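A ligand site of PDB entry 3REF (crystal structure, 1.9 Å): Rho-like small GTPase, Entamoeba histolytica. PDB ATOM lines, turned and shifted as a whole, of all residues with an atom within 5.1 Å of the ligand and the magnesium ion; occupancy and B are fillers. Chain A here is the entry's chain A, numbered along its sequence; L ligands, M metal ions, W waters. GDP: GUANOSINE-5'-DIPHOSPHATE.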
ATOM      1  N   ASP A  31       9.526  15.654 -12.337  1.00  0.00           N
ATOM      2  CA  ASP A  31       8.473  16.609 -12.696  1.00  0.00           C
ATOM      3  C   ASP A  31       7.385  16.011 -13.602  1.00  0.00           C
ATOM      4  O   ASP A  31       7.644  15.097 -14.402  1.00  0.00           O
ATOM      5  CB  ASP A  31       9.076  17.815 -13.425  1.00  0.00           C
ATOM      6  CG  ASP A  31       9.859  18.733 -12.503  1.00  0.00           C
ATOM      7  OD1 ASP A  31      10.034  18.429 -11.287  1.00  0.00           O
ATOM      8  OD2 ASP A  31      10.317  19.781 -13.004  1.00  0.00           O
ATOM      9  N   GLY A  32       6.184  16.561 -13.507  1.00  0.00           N
ATOM     10  CA  GLY A  32       5.138  16.194 -14.450  1.00  0.00           C
ATOM     11  C   GLY A  32       5.601  16.452 -15.882  1.00  0.00           C
ATOM     12  O   GLY A  32       6.366  17.386 -16.152  1.00  0.00           O
ATOM     13  N   ALA A  33       5.132  15.608 -16.796  1.00  0.00           N
ATOM     14  CA  ALA A  33       5.418  15.743 -18.212  1.00  0.00           C
ATOM     15  C   ALA A  33       6.893  15.475 -18.629  1.00  0.00           C
ATOM     16  O   ALA A  33       7.259  15.764 -19.753  1.00  0.00           O
ATOM     17  CB  ALA A  33       4.964  17.135 -18.711  1.00  0.00           C
ATOM     18  N   VAL A  34       7.738  14.897 -17.770  1.00  0.00           N
ATOM     19  CA  VAL A  34       9.082  14.555 -18.253  1.00  0.00           C
ATOM     20  C   VAL A  34       9.067  13.220 -19.037  1.00  0.00           C
ATOM     21  O   VAL A  34      10.007  12.911 -19.792  1.00  0.00           O
ATOM     22  CB  VAL A  34      10.139  14.500 -17.152  1.00  0.00           C
ATOM     23  CG1 VAL A  34      10.191  15.837 -16.385  1.00  0.00           C
ATOM     24  CG2 VAL A  34       9.894  13.293 -16.222  1.00  0.00           C
ATOM     25  N   GLY A  35       8.007  12.448 -18.871  1.00  0.00           N
ATOM     26  CA  GLY A  35       7.824  11.194 -19.605  1.00  0.00           C
ATOM     27  C   GLY A  35       7.878   9.891 -18.803  1.00  0.00           C
ATOM     28  O   GLY A  35       8.207   8.838 -19.332  1.00  0.00           O
ATOM     29  N   LYS A  36       7.565   9.967 -17.509  1.00  0.00           N
ATOM     30  CA  LYS A  36       7.635   8.811 -16.635  1.00  0.00           C
ATOM     31  C   LYS A  36       6.649   7.690 -17.004  1.00  0.00           C
ATOM     32  O   LYS A  36       7.013   6.528 -17.067  1.00  0.00           O
ATOM     33  CB  LYS A  36       7.398   9.255 -15.174  1.00  0.00           C
ATOM     34  CG  LYS A  36       8.411  10.305 -14.663  1.00  0.00           C
ATOM     35  CD  LYS A  36       8.194  10.713 -13.162  1.00  0.00           C
ATOM     36  CE  LYS A  36       6.797  11.269 -12.895  1.00  0.00           C
ATOM     37  NZ  LYS A  36       6.562  12.528 -13.699  1.00  0.00           N
ATOM     38  N   THR A  37       5.383   8.044 -17.246  1.00  0.00           N
ATOM     39  CA  THR A  37       4.402   7.026 -17.592  1.00  0.00           C
ATOM     40  C   THR A  37       4.731   6.393 -18.962  1.00  0.00           C
ATOM     41  O   THR A  37       4.630   5.190 -19.135  1.00  0.00           O
ATOM     42  CB  THR A  37       2.962   7.595 -17.551  1.00  0.00           C
ATOM     43  OG1 THR A  37       2.698   8.098 -16.231  1.00  0.00           O
ATOM     44  CG2 THR A  37       1.900   6.501 -17.887  1.00  0.00           C
ATOM     45  N   CYS A  38       5.138   7.218 -19.925  1.00  0.00           N
ATOM     46  CA  CYS A  38       5.531   6.694 -21.245  1.00  0.00           C
ATOM     47  C   CYS A  38       6.779   5.797 -21.167  1.00  0.00           C
ATOM     48  O   CYS A  38       6.901   4.835 -21.914  1.00  0.00           O
ATOM     49  CB  CYS A  38       5.744   7.845 -22.231  1.00  0.00           C
ATOM     50  SG  CYS A  38       4.179   8.630 -22.763  1.00  0.00           S
ATOM     51  N   LEU A  39       7.706   6.111 -20.276  1.00  0.00           N
ATOM     52  CA  LEU A  39       8.858   5.255 -20.061  1.00  0.00           C
ATOM     53  C   LEU A  39       8.403   3.859 -19.663  1.00  0.00           C
ATOM     54  O   LEU A  39       8.861   2.882 -20.254  1.00  0.00           O
ATOM     55  CB  LEU A  39       9.805   5.822 -18.997  1.00  0.00           C
ATOM     56  CG  LEU A  39      10.892   4.846 -18.534  1.00  0.00           C
ATOM     57  CD1 LEU A  39      11.837   4.563 -19.709  1.00  0.00           C
ATOM     58  CD2 LEU A  39      11.660   5.449 -17.340  1.00  0.00           C
ATOM     59  N   ILE A  48       3.889   3.099 -27.087  1.00  0.00           N
ATOM     60  CA  ILE A  48       3.052   4.026 -26.362  1.00  0.00           C
ATOM     61  C   ILE A  48       1.714   3.993 -27.082  1.00  0.00           C
ATOM     62  O   ILE A  48       1.638   4.347 -28.255  1.00  0.00           O
ATOM     63  CB  ILE A  48       3.639   5.454 -26.392  1.00  0.00           C
ATOM     64  CG1 ILE A  48       5.075   5.444 -25.838  1.00  0.00           C
ATOM     65  CG2 ILE A  48       2.737   6.428 -25.634  1.00  0.00           C
ATOM     66  CD1 ILE A  48       5.833   6.742 -26.057  1.00  0.00           C
ATOM     67  N   VAL A  53      -3.681   8.333 -21.894  1.00  0.00           N
ATOM     68  CA  VAL A  53      -2.581   7.936 -21.018  1.00  0.00           C
ATOM     69  C   VAL A  53      -2.882   8.422 -19.602  1.00  0.00           C
ATOM     70  O   VAL A  53      -3.141   9.602 -19.379  1.00  0.00           O
ATOM     71  CB  VAL A  53      -1.248   8.527 -21.503  1.00  0.00           C
ATOM     72  CG1 VAL A  53      -1.430   9.985 -21.921  1.00  0.00           C
ATOM     73  CG2 VAL A  53      -0.181   8.381 -20.424  1.00  0.00           C
ATOM     74  N   PRO A  54      -2.867   7.488 -18.632  1.00  0.00           N
ATOM     75  CA  PRO A  54      -3.273   7.824 -17.254  1.00  0.00           C
ATOM     76  C   PRO A  54      -2.242   8.735 -16.598  1.00  0.00           C
ATOM     77  O   PRO A  54      -1.095   8.743 -17.028  1.00  0.00           O
ATOM     78  CB  PRO A  54      -3.290   6.460 -16.556  1.00  0.00           C
ATOM     79  CG  PRO A  54      -2.261   5.656 -17.296  1.00  0.00           C
ATOM     80  CD  PRO A  54      -2.354   6.113 -18.740  1.00  0.00           C
ATOM     81  N   THR A  55      -2.653   9.480 -15.577  1.00  0.00           N
ATOM     82  CA  THR A  55      -1.716  10.309 -14.835  1.00  0.00           C
ATOM     83  C   THR A  55      -0.682   9.401 -14.180  1.00  0.00           C
ATOM     84  O   THR A  55       0.514   9.634 -14.276  1.00  0.00           O
ATOM     85  CB  THR A  55      -2.425  11.127 -13.735  1.00  0.00           C
ATOM     86  OG1 THR A  55      -3.432  11.961 -14.325  1.00  0.00           O
ATOM     87  CG2 THR A  55      -1.429  11.991 -12.980  1.00  0.00           C
ATOM     88  N   VAL A  56      -1.170   8.351 -13.512  1.00  0.00           N
ATOM     89  CA  VAL A  56      -0.290   7.369 -12.892  1.00  0.00           C
ATOM     90  C   VAL A  56      -0.731   5.961 -13.203  1.00  0.00           C
ATOM     91  O   VAL A  56      -1.856   5.565 -12.900  1.00  0.00           O
ATOM     92  CB  VAL A  56      -0.235   7.528 -11.350  1.00  0.00           C
ATOM     93  CG1 VAL A  56       0.498   6.335 -10.726  1.00  0.00           C
ATOM     94  CG2 VAL A  56       0.459   8.828 -10.985  1.00  0.00           C
ATOM     95  N   ASP A  77       4.945   3.848 -10.937  1.00  0.00           N
ATOM     96  CA  ASP A  77       4.837   5.182 -11.503  1.00  0.00           C
ATOM     97  C   ASP A  77       4.430   6.076 -10.348  1.00  0.00           C
ATOM     98  O   ASP A  77       3.923   5.568  -9.355  1.00  0.00           O
ATOM     99  CB  ASP A  77       3.735   5.125 -12.568  1.00  0.00           C
ATOM    100  CG  ASP A  77       3.708   6.333 -13.483  1.00  0.00           C
ATOM    101  OD1 ASP A  77       4.613   7.180 -13.378  1.00  0.00           O
ATOM    102  OD2 ASP A  77       2.787   6.414 -14.323  1.00  0.00           O
ATOM    103  N   THR A  78       4.684   7.375 -10.441  1.00  0.00           N
ATOM    104  CA  THR A  78       4.262   8.371  -9.428  1.00  0.00           C
ATOM    105  C   THR A  78       3.901   9.666 -10.147  1.00  0.00           C
ATOM    106  O   THR A  78       4.251   9.852 -11.310  1.00  0.00           O
ATOM    107  CB  THR A  78       5.379   8.737  -8.414  1.00  0.00           C
ATOM    108  OG1 THR A  78       6.420   9.476  -9.079  1.00  0.00           O
ATOM    109  CG2 THR A  78       5.945   7.495  -7.726  1.00  0.00           C
ATOM    110  N   ALA A  79       3.253  10.576  -9.444  1.00  0.00           N
ATOM    111  CA  ALA A  79       2.968  11.905 -10.022  1.00  0.00           C
ATOM    112  C   ALA A  79       2.877  12.940  -8.934  1.00  0.00           C
ATOM    113  O   ALA A  79       3.014  12.611  -7.749  1.00  0.00           O
ATOM    114  CB  ALA A  79       1.687  11.882 -10.816  1.00  0.00           C
ATOM    115  N   LYS A 136      13.214  11.727 -23.141  1.00  0.00           N
ATOM    116  CA  LYS A 136      12.966  12.456 -24.388  1.00  0.00           C
ATOM    117  C   LYS A 136      14.253  12.849 -25.109  1.00  0.00           C
ATOM    118  O   LYS A 136      14.322  13.920 -25.736  1.00  0.00           O
ATOM    119  CB  LYS A 136      12.160  13.729 -24.120  1.00  0.00           C
ATOM    120  CG  LYS A 136      10.926  13.531 -23.233  1.00  0.00           C
ATOM    121  CD  LYS A 136       9.945  14.713 -23.419  1.00  0.00           C
ATOM    122  CE  LYS A 136       8.712  14.576 -22.529  1.00  0.00           C
ATOM    123  NZ  LYS A 136       7.879  15.820 -22.532  1.00  0.00           N
ATOM    124  N   ASP A 138      15.372  11.960 -27.843  1.00  0.00           N
ATOM    125  CA  ASP A 138      15.079  12.203 -29.253  1.00  0.00           C
ATOM    126  C   ASP A 138      14.876  13.687 -29.553  1.00  0.00           C
ATOM    127  O   ASP A 138      14.978  14.105 -30.711  1.00  0.00           O
ATOM    128  CB  ASP A 138      13.833  11.410 -29.709  1.00  0.00           C
ATOM    129  CG  ASP A 138      12.592  11.788 -28.925  1.00  0.00           C
ATOM    130  OD1 ASP A 138      12.477  11.400 -27.735  1.00  0.00           O
ATOM    131  OD2 ASP A 138      11.736  12.493 -29.493  1.00  0.00           O
ATOM    132  N   LEU A 139      14.589  14.482 -28.522  1.00  0.00           N
ATOM    133  CA  LEU A 139      14.265  15.904 -28.703  1.00  0.00           C
ATOM    134  C   LEU A 139      15.484  16.821 -28.655  1.00  0.00           C
ATOM    135  O   LEU A 139      15.366  17.987 -28.986  1.00  0.00           O
ATOM    136  CB  LEU A 139      13.252  16.376 -27.638  1.00  0.00           C
ATOM    137  CG  LEU A 139      11.846  15.771 -27.779  1.00  0.00           C
ATOM    138  CD1 LEU A 139      10.895  16.302 -26.667  1.00  0.00           C
ATOM    139  CD2 LEU A 139      11.316  16.098 -29.175  1.00  0.00           C
ATOM    140  N   ALA A 167      17.384   8.212 -22.599  1.00  0.00           N
ATOM    141  CA  ALA A 167      16.382   7.307 -23.188  1.00  0.00           C
ATOM    142  C   ALA A 167      15.333   8.087 -23.958  1.00  0.00           C
ATOM    143  O   ALA A 167      15.129   9.272 -23.715  1.00  0.00           O
ATOM    144  CB  ALA A 167      15.728   6.462 -22.100  1.00  0.00           C
ATOM    145  N   SER A 168      14.705   7.419 -24.920  1.00  0.00           N
ATOM    146  CA  SER A 168      13.539   7.963 -25.603  1.00  0.00           C
ATOM    147  C   SER A 168      12.491   6.854 -25.716  1.00  0.00           C
ATOM    148  O   SER A 168      12.710   5.835 -26.379  1.00  0.00           O
ATOM    149  CB  SER A 168      13.874   8.454 -27.012  1.00  0.00           C
ATOM    150  OG  SER A 168      12.667   8.785 -27.688  1.00  0.00           O
ATOM    151  N   SER A 169      11.368   7.053 -25.046  1.00  0.00           N
ATOM    152  CA  SER A 169      10.236   6.138 -25.178  1.00  0.00           C
ATOM    153  C   SER A 169       9.692   6.121 -26.586  1.00  0.00           C
ATOM    154  O   SER A 169       9.246   5.093 -27.082  1.00  0.00           O
ATOM    155  CB  SER A 169       9.115   6.585 -24.228  1.00  0.00           C
ATOM    156  OG  SER A 169       9.561   6.479 -22.895  1.00  0.00           O
ATOM    157  N   VAL A 170       9.678   7.276 -27.233  1.00  0.00           N
ATOM    158  CA  VAL A 170       9.096   7.392 -28.574  1.00  0.00           C
ATOM    159  C   VAL A 170       9.990   6.690 -29.618  1.00  0.00           C
ATOM    160  O   VAL A 170       9.522   5.882 -30.434  1.00  0.00           O
ATOM    161  CB  VAL A 170       8.868   8.881 -28.919  1.00  0.00           C
ATOM    162  CG1 VAL A 170       8.657   9.085 -30.404  1.00  0.00           C
ATOM    163  CG2 VAL A 170       7.684   9.447 -28.075  1.00  0.00           C
ATOM    164  N   ALA A 171      11.293   6.963 -29.534  1.00  0.00           N
ATOM    165  CA  ALA A 171      12.259   6.422 -30.501  1.00  0.00           C
ATOM    166  C   ALA A 171      12.792   5.036 -30.158  1.00  0.00           C
ATOM    167  O   ALA A 171      13.512   4.437 -30.969  1.00  0.00           O
ATOM    168  CB  ALA A 171      13.412   7.399 -30.705  1.00  0.00           C
HETATM  169  PB  GDP L   1       4.792  12.089 -16.920  1.00  0.00           P
HETATM  170  O1B GDP L   1       6.237  12.277 -16.410  1.00  0.00           O
HETATM  171  O2B GDP L   1       3.940  13.183 -16.398  1.00  0.00           O
HETATM  172  O3B GDP L   1       4.380  10.692 -16.596  1.00  0.00           O
HETATM  173  O3A GDP L   1       4.893  12.279 -18.529  1.00  0.00           O
HETATM  174  PA  GDP L   1       4.174  11.295 -19.611  1.00  0.00           P
HETATM  175  O1A GDP L   1       2.680  11.367 -19.413  1.00  0.00           O
HETATM  176  O2A GDP L   1       4.737   9.927 -19.657  1.00  0.00           O
HETATM  177  O5' GDP L   1       4.615  12.141 -20.928  1.00  0.00           O
HETATM  178  C5' GDP L   1       4.197  13.485 -21.114  1.00  0.00           C
HETATM  179  C4' GDP L   1       4.239  13.757 -22.620  1.00  0.00           C
HETATM  180  O4' GDP L   1       5.580  13.736 -23.113  1.00  0.00           O
HETATM  181  C3' GDP L   1       3.489  12.690 -23.394  1.00  0.00           C
HETATM  182  O3' GDP L   1       2.272  13.263 -23.871  1.00  0.00           O
HETATM  183  C2' GDP L   1       4.308  12.462 -24.643  1.00  0.00           C
HETATM  184  O2' GDP L   1       3.639  13.193 -25.677  1.00  0.00           O
HETATM  185  C1' GDP L   1       5.641  13.149 -24.400  1.00  0.00           C
HETATM  186  N9  GDP L   1       6.723  12.165 -24.384  1.00  0.00           N
HETATM  187  C8  GDP L   1       6.903  11.190 -23.466  1.00  0.00           C
HETATM  188  N7  GDP L   1       8.035  10.483 -23.745  1.00  0.00           N
HETATM  189  C5  GDP L   1       8.565  11.036 -24.866  1.00  0.00           C
HETATM  190  C6  GDP L   1       9.757  10.801 -25.706  1.00  0.00           C
HETATM  191  O6  GDP L   1      10.533   9.861 -25.433  1.00  0.00           O
HETATM  192  N1  GDP L   1       9.961  11.606 -26.760  1.00  0.00           N
HETATM  193  C2  GDP L   1       9.113  12.619 -27.073  1.00  0.00           C
HETATM  194  N2  GDP L   1       9.359  13.384 -28.157  1.00  0.00           N
HETATM  195  N3  GDP L   1       8.015  12.893 -26.354  1.00  0.00           N
HETATM  196  C4  GDP L   1       7.697  12.142 -25.279  1.00  0.00           C
HETATM  197 MG    MG M   1       2.391  10.282 -15.469  1.00  0.00          MG
HETATM  198  O   HOH W   1       2.016  14.529 -18.000  1.00  0.00           O
HETATM  199  O   HOH W   2      11.673   9.229 -23.188  1.00  0.00           O
HETATM  200  O   HOH W   3       3.662   9.616 -13.949  1.00  0.00           O
HETATM  201  O   HOH W   4       4.016  13.186 -13.001  1.00  0.00           O
HETATM  202  O   HOH W   5       1.254  10.461 -17.234  1.00  0.00           O
HETATM  203  O   HOH W   6       0.442  12.084 -20.423  1.00  0.00           O
HETATM  204  O   HOH W   7       9.371   8.814 -21.780  1.00  0.00           O
HETATM  205  O   HOH W   8       2.120  12.502 -14.819  1.00  0.00           O
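An oxygen (O2A) of the ligand lies within hydrogen-bond range of the backbone NH (N) of Thr 37, 3.1 Å away.
A nitrogen (N1) of the ligand sits at hydrogen-bond distance from the side-chain carboxylate of Asp 138 (2.7 Å).
An oxygen (O2B) of the ligand sits at hydrogen-bond distance from the backbone NH of Ala 33 (2.7 Å).
N of Lys 36 sits at hydrogen-bond distance from O1B of the ligand (2.9 Å).
An oxygen (O1B) of the ligand is in salt-bridge range of the side-chain amino group (NZ) of Lys 36, at 2.7 Å.
N of Cys 38 is in hydrogen-bond range of O2A of the ligand (2.8 Å).
The side-chain sulfur (SG) of Cys 38 sits at hydrogen-bond distance from an oxygen (O2A) of the ligand, 3.4 Å away.
The backbone NH (N) of Ser 169 is in hydrogen-bond range of an oxygen (O6) of the ligand, at 3.0 Å.
The backbone NH (N) of Gly 35 is in hydrogen-bond range of an oxygen (O1B) of the ligand, at 3.0 Å.
O4' of the ligand sits at hydrogen-bond distance from NZ of Lys 136, at 3.2 Å.
The backbone NH (N) of Val 170 sits at hydrogen-bond distance from an oxygen (O6) of the ligand (3.3 Å).
An oxygen (O6) of the ligand is in hydrogen-bond range of the side-chain hydroxyl (OG) of Ser 168 (3.3 Å).
O1B of the ligand is in hydrogen-bond range of N of Val 34, at 3.3 Å.
OG1 of Thr 37 lies close to OD2 of Asp 77.
The side-chain carboxylate (OD1) of Asp 138 sits at hydrogen-bond distance from the side-chain hydroxyl (OG) of Ser 168 (2.6 Å).
The backbone carbonyl oxygen of Ala 33 sits at hydrogen-bond distance from the side-chain amino group of Lys 136, at 2.8 Å.
The side-chain hydroxyl (OG) of Ser 169 sits at hydrogen-bond distance from the backbone carbonyl oxygen (O) of Cys 38.
The side-chain hydroxyl of Ser 169 lies close to the backbone NH of Leu 39, at 3.2 Å.
The backbone carbonyl oxygen of Ala 167 sits at hydrogen-bond distance from the backbone NH of Lys 136 (3.2 Å).
The backbone NH (N) of Val 170 sits close to the side-chain hydroxyl (OG) of Ser 168 (3.4 Å).
OG of Ser 168 lies within hydrogen-bond range of N of Ala 171, at 2.9 Å.
Merely in contact with the ligand: Asp 31 (3.7 Å), Gly 32 (3.7 Å) and Leu 139 (3.5 Å).
Hydrophobic or aromatic side chains within 4 Å of the ligand: Val 34, Leu 139 and Val 170.
Of the 25 residues printed, 14 come within 4 Å of the ligand.
Of the 25 residues printed, 2 come within 4 Å of the magnesium ion.
Water W3 binds the magnesium ion (2.1 Å).
Water W5 binds the magnesium ion (2.1 Å).
The magnesium ion is bound by O of Thr 55, at 2.3 Å.
An oxygen (O3B) of the ligand binds the magnesium ion (2.3 Å).
The magnesium ion is bound by water W8.
The magnesium ion is bound by OG1 of Thr 37, at 2.3 Å.
The magnesium ion has six donor atoms within binding distance.
Water W3 lies within hydrogen-bond range of the side-chain carboxylate (OD1) of Asp 77 (2.7 Å) and the backbone carbonyl oxygen (O) of Thr 78 (2.7 Å).
Water W5 bridges O1A of the ligand (2.8 Å) and O of Pro 54 (2.9 Å).
Water W2 lies within hydrogen-bond range of an oxygen (O6) of the ligand (2.6 Å), the backbone NH of Ser 169 (2.9 Å), the backbone NH of Lys 136 (2.9 Å) and the backbone carbonyl oxygen of Ala 167 (3.5 Å).
Water W7 lies within hydrogen-bond range of the side-chain hydroxyl (OG) of Ser 169, the backbone carbonyl oxygen (O) of Gly 35 and a nitrogen (N7) of the ligand.
Water W4 bridges the side-chain amino group (NZ) of Lys 36 (2.7 Å) and an oxygen (O2B) of the ligand (3.4 Å).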
